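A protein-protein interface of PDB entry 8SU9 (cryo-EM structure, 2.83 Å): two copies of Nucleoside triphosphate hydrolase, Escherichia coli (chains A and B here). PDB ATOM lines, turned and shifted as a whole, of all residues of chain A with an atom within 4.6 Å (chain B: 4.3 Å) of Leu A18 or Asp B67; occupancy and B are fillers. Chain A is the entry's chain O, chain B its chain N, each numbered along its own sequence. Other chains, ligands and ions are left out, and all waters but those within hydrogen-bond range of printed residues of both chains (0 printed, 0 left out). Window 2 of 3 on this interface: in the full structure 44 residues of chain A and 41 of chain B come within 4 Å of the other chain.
O of Met B68 sits at hydrogen-bond distance from N of Leu A18 (3.0 Å).
OD1 of Asp B67 is in hydrogen-bond range of N of Gly A20.
The backbone NH (N) of Thr B66 is in hydrogen-bond range of the backbone carbonyl oxygen (O) of Ile B95 (2.9 Å).
The backbone NH (N) of Ile B95 lies within hydrogen-bond range of the backbone carbonyl oxygen (O) of Asp B67 (3.3 Å).
Among the printed residues, pairs that only touch across the chains: Gly A17 with Met B68, Leu A18 with Asp B67, Glu A19 with Asp B67, Gly A20 with Pro B48 and Gly A20 with Thr B66.
Of the printed residues of chain B, Gly A17 touches Met B68 (3.8 Å).
Of chain B, only Asp B67 (3.8 Å) and Met B68 (3.0 Å) come within 4 Å of Leu A18.
Of the printed residues of chain B, Gly A20 touches Pro B48, Thr B66 and Asp B67.
Leu A118 touches none of the printed residues of chain B.
Printed residues of chain A within 4 Å of Thr B66: Gly A20.
Asp B67 touches three residues of chain A.
Ile B95 touches none of the printed residues of chain A.
The nearest printed residue of chain A that does not touch Asp B67 is Gly A17 (7.4 Å).
The nearest printed residue of chain B that does not touch Gly A20 is Met B68 (6.4 Å).
Of the 8 printed residues of chain B, 4 touch a printed residue of chain A.
Of the 9 printed residues of chain A, 4 touch a printed residue of chain B.
Printed residues of chain A that touch a printed residue of chain B: Gly A17, Leu A18, Glu A19 and Gly A20.
Among the printed residues, no Asp or Glu carboxylate lies within 4 Å of a Lys or Arg side-chain nitrogen of the other chain.
No position is printed for both chains.
Of the 7 pairs that touch across the chains among the printed residues, none has its exchanged pair printed and touching as well.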
ATOM      1  N   GLY A  17     -20.806 -15.901 -19.498  1.00  0.00           N
ATOM      2  CA  GLY A  17     -21.677 -15.140 -20.376  1.00  0.00           C
ATOM      3  C   GLY A  17     -20.949 -14.533 -21.552  1.00  0.00           C
ATOM      4  O   GLY A  17     -19.727 -14.358 -21.534  1.00  0.00           O
ATOM      5  N   LEU A  18     -21.727 -14.205 -22.586  1.00  0.00           N
ATOM      6  CA  LEU A  18     -21.222 -13.563 -23.802  1.00  0.00           C
ATOM      7  C   LEU A  18     -22.288 -12.585 -24.289  1.00  0.00           C
ATOM      8  O   LEU A  18     -23.255 -12.992 -24.938  1.00  0.00           O
ATOM      9  CB  LEU A  18     -20.892 -14.583 -24.885  1.00  0.00           C
ATOM     10  CG  LEU A  18     -19.718 -15.545 -24.721  1.00  0.00           C
ATOM     11  CD1 LEU A  18     -19.804 -16.628 -25.775  1.00  0.00           C
ATOM     12  CD2 LEU A  18     -18.399 -14.808 -24.817  1.00  0.00           C
ATOM     13  N   GLU A  19     -22.110 -11.303 -23.981  1.00  0.00           N
ATOM     14  CA  GLU A  19     -23.049 -10.256 -24.369  1.00  0.00           C
ATOM     15  C   GLU A  19     -22.360  -9.344 -25.373  1.00  0.00           C
ATOM     16  O   GLU A  19     -21.393  -8.655 -25.032  1.00  0.00           O
ATOM     17  CB  GLU A  19     -23.526  -9.466 -23.151  1.00  0.00           C
ATOM     18  CG  GLU A  19     -24.372 -10.268 -22.175  1.00  0.00           C
ATOM     19  CD  GLU A  19     -23.535 -11.080 -21.205  1.00  0.00           C
ATOM     20  OE1 GLU A  19     -22.291 -10.975 -21.256  1.00  0.00           O
ATOM     21  OE2 GLU A  19     -24.121 -11.824 -20.390  1.00  0.00           O
ATOM     22  N   GLY A  20     -22.863  -9.330 -26.606  1.00  0.00           N
ATOM     23  CA  GLY A  20     -22.225  -8.569 -27.660  1.00  0.00           C
ATOM     24  C   GLY A  20     -20.833  -9.083 -27.948  1.00  0.00           C
ATOM     25  O   GLY A  20     -20.665 -10.159 -28.526  1.00  0.00           O
ATOM     26  N   ARG A  22     -18.384  -8.466 -25.220  1.00  0.00           N
ATOM     27  CA  ARG A  22     -17.822  -8.600 -23.884  1.00  0.00           C
ATOM     28  C   ARG A  22     -17.881 -10.044 -23.398  1.00  0.00           C
ATOM     29  O   ARG A  22     -18.714 -10.840 -23.835  1.00  0.00           O
ATOM     30  CB  ARG A  22     -18.573  -7.698 -22.908  1.00  0.00           C
ATOM     31  CG  ARG A  22     -18.759  -6.281 -23.400  1.00  0.00           C
ATOM     32  CD  ARG A  22     -19.827  -5.558 -22.602  1.00  0.00           C
ATOM     33  NE  ARG A  22     -19.303  -4.983 -21.371  1.00  0.00           N
ATOM     34  CZ  ARG A  22     -20.057  -4.495 -20.396  1.00  0.00           C
ATOM     35  NH1 ARG A  22     -21.378  -4.503 -20.474  1.00  0.00           N
ATOM     36  NH2 ARG A  22     -19.472  -3.987 -19.315  1.00  0.00           N
ATOM     37  N   ILE A  23     -16.978 -10.376 -22.477  1.00  0.00           N
ATOM     38  CA  ILE A  23     -16.900 -11.695 -21.863  1.00  0.00           C
ATOM     39  C   ILE A  23     -16.990 -11.530 -20.352  1.00  0.00           C
ATOM     40  O   ILE A  23     -16.385 -10.615 -19.786  1.00  0.00           O
ATOM     41  CB  ILE A  23     -15.602 -12.434 -22.253  1.00  0.00           C
ATOM     42  CG1 ILE A  23     -15.413 -12.419 -23.770  1.00  0.00           C
ATOM     43  CG2 ILE A  23     -15.618 -13.858 -21.733  1.00  0.00           C
ATOM     44  CD1 ILE A  23     -14.010 -12.745 -24.213  1.00  0.00           C
ATOM     45  N   LEU A 118     -14.722 -15.797 -30.251  1.00  0.00           N
ATOM     46  CA  LEU A 118     -14.970 -15.781 -28.820  1.00  0.00           C
ATOM     47  C   LEU A 118     -14.999 -17.209 -28.303  1.00  0.00           C
ATOM     48  O   LEU A 118     -15.328 -18.139 -29.047  1.00  0.00           O
ATOM     49  CB  LEU A 118     -16.291 -15.076 -28.487  1.00  0.00           C
ATOM     50  CG  LEU A 118     -16.434 -13.623 -28.936  1.00  0.00           C
ATOM     51  CD1 LEU A 118     -17.821 -13.106 -28.618  1.00  0.00           C
ATOM     52  CD2 LEU A 118     -15.380 -12.757 -28.279  1.00  0.00           C
ATOM     53  N   PRO A 119     -14.655 -17.418 -27.036  1.00  0.00           N
ATOM     54  CA  PRO A 119     -14.723 -18.763 -26.460  1.00  0.00           C
ATOM     55  C   PRO A 119     -16.152 -19.172 -26.137  1.00  0.00           C
ATOM     56  O   PRO A 119     -17.061 -18.349 -26.028  1.00  0.00           O
ATOM     57  CB  PRO A 119     -13.884 -18.642 -25.186  1.00  0.00           C
ATOM     58  CG  PRO A 119     -13.997 -17.211 -24.807  1.00  0.00           C
ATOM     59  CD  PRO A 119     -14.105 -16.436 -26.084  1.00  0.00           C
ATOM     60  N   LEU A 121     -19.197 -21.159 -23.841  1.00  0.00           N
ATOM     61  CA  LEU A 121     -19.614 -21.131 -22.446  1.00  0.00           C
ATOM     62  C   LEU A 121     -19.044 -22.324 -21.690  1.00  0.00           C
ATOM     63  O   LEU A 121     -19.075 -23.458 -22.177  1.00  0.00           O
ATOM     64  CB  LEU A 121     -21.139 -21.128 -22.354  1.00  0.00           C
ATOM     65  CG  LEU A 121     -21.824 -19.773 -22.181  1.00  0.00           C
ATOM     66  CD1 LEU A 121     -21.538 -18.866 -23.361  1.00  0.00           C
ATOM     67  CD2 LEU A 121     -23.316 -19.964 -22.005  1.00  0.00           C
ATOM     68  N   PRO B  48     -22.261 -15.228 -30.727  1.00  0.00           N
ATOM     69  CA  PRO B  48     -23.066 -14.192 -31.382  1.00  0.00           C
ATOM     70  C   PRO B  48     -22.559 -13.884 -32.783  1.00  0.00           C
ATOM     71  O   PRO B  48     -21.357 -13.906 -33.051  1.00  0.00           O
ATOM     72  CB  PRO B  48     -22.910 -12.984 -30.454  1.00  0.00           C
ATOM     73  CG  PRO B  48     -22.610 -13.568 -29.129  1.00  0.00           C
ATOM     74  CD  PRO B  48     -21.807 -14.804 -29.390  1.00  0.00           C
ATOM     75  N   VAL B  65     -28.028 -14.164 -33.952  1.00  0.00           N
ATOM     76  CA  VAL B  65     -27.819 -14.318 -32.514  1.00  0.00           C
ATOM     77  C   VAL B  65     -27.137 -13.076 -31.957  1.00  0.00           C
ATOM     78  O   VAL B  65     -26.271 -12.482 -32.607  1.00  0.00           O
ATOM     79  CB  VAL B  65     -26.993 -15.584 -32.220  1.00  0.00           C
ATOM     80  CG1 VAL B  65     -26.964 -15.872 -30.731  1.00  0.00           C
ATOM     81  CG2 VAL B  65     -27.554 -16.766 -32.983  1.00  0.00           C
ATOM     82  N   THR B  66     -27.524 -12.680 -30.741  1.00  0.00           N
ATOM     83  CA  THR B  66     -26.942 -11.504 -30.100  1.00  0.00           C
ATOM     84  C   THR B  66     -26.379 -11.800 -28.713  1.00  0.00           C
ATOM     85  O   THR B  66     -25.346 -11.239 -28.335  1.00  0.00           O
ATOM     86  CB  THR B  66     -27.977 -10.381 -29.996  1.00  0.00           C
ATOM     87  OG1 THR B  66     -29.078 -10.817 -29.190  1.00  0.00           O
ATOM     88  CG2 THR B  66     -28.486  -9.987 -31.369  1.00  0.00           C
ATOM     89  N   ASP B  67     -27.035 -12.668 -27.941  1.00  0.00           N
ATOM     90  CA  ASP B  67     -26.661 -12.889 -26.549  1.00  0.00           C
ATOM     91  C   ASP B  67     -26.722 -14.370 -26.200  1.00  0.00           C
ATOM     92  O   ASP B  67     -27.518 -15.131 -26.756  1.00  0.00           O
ATOM     93  CB  ASP B  67     -27.564 -12.097 -25.597  1.00  0.00           C
ATOM     94  CG  ASP B  67     -27.254 -10.615 -25.594  1.00  0.00           C
ATOM     95  OD1 ASP B  67     -26.080 -10.251 -25.813  1.00  0.00           O
ATOM     96  OD2 ASP B  67     -28.184  -9.812 -25.375  1.00  0.00           O
ATOM     97  N   MET B  68     -25.862 -14.767 -25.260  1.00  0.00           N
ATOM     98  CA  MET B  68     -25.827 -16.113 -24.701  1.00  0.00           C
ATOM     99  C   MET B  68     -25.417 -16.008 -23.239  1.00  0.00           C
ATOM    100  O   MET B  68     -24.460 -15.298 -22.918  1.00  0.00           O
ATOM    101  CB  MET B  68     -24.837 -17.020 -25.447  1.00  0.00           C
ATOM    102  CG  MET B  68     -24.967 -17.034 -26.957  1.00  0.00           C
ATOM    103  SD  MET B  68     -23.925 -18.280 -27.732  1.00  0.00           S
ATOM    104  CE  MET B  68     -24.685 -19.777 -27.121  1.00  0.00           C
ATOM    105  N   GLN B  93     -29.680 -19.894 -22.414  1.00  0.00           N
ATOM    106  CA  GLN B  93     -30.653 -19.093 -23.145  1.00  0.00           C
ATOM    107  C   GLN B  93     -29.968 -18.334 -24.274  1.00  0.00           C
ATOM    108  O   GLN B  93     -28.750 -18.136 -24.269  1.00  0.00           O
ATOM    109  CB  GLN B  93     -31.376 -18.106 -22.222  1.00  0.00           C
ATOM    110  CG  GLN B  93     -32.660 -18.635 -21.625  1.00  0.00           C
ATOM    111  CD  GLN B  93     -33.509 -17.541 -21.021  1.00  0.00           C
ATOM    112  OE1 GLN B  93     -33.137 -16.370 -21.039  1.00  0.00           O
ATOM    113  NE2 GLN B  93     -34.658 -17.918 -20.478  1.00  0.00           N
ATOM    114  N   ILE B  94     -30.776 -17.902 -25.248  1.00  0.00           N
ATOM    115  CA  ILE B  94     -30.302 -17.204 -26.437  1.00  0.00           C
ATOM    116  C   ILE B  94     -31.309 -16.122 -26.814  1.00  0.00           C
ATOM    117  O   ILE B  94     -32.522 -16.302 -26.696  1.00  0.00           O
ATOM    118  CB  ILE B  94     -30.079 -18.181 -27.621  1.00  0.00           C
ATOM    119  CG1 ILE B  94     -28.832 -19.032 -27.395  1.00  0.00           C
ATOM    120  CG2 ILE B  94     -29.960 -17.444 -28.945  1.00  0.00           C
ATOM    121  CD1 ILE B  94     -28.514 -19.956 -28.545  1.00  0.00           C
ATOM    122  N   ILE B  95     -30.788 -14.978 -27.268  1.00  0.00           N
ATOM    123  CA  ILE B  95     -31.595 -13.873 -27.775  1.00  0.00           C
ATOM    124  C   ILE B  95     -31.240 -13.639 -29.240  1.00  0.00           C
ATOM    125  O   ILE B  95     -30.066 -13.668 -29.622  1.00  0.00           O
ATOM    126  CB  ILE B  95     -31.388 -12.583 -26.950  1.00  0.00           C
ATOM    127  CG1 ILE B  95     -31.765 -12.815 -25.489  1.00  0.00           C
ATOM    128  CG2 ILE B  95     -32.208 -11.442 -27.514  1.00  0.00           C
ATOM    129  CD1 ILE B  95     -33.212 -13.187 -25.286  1.00  0.00           C
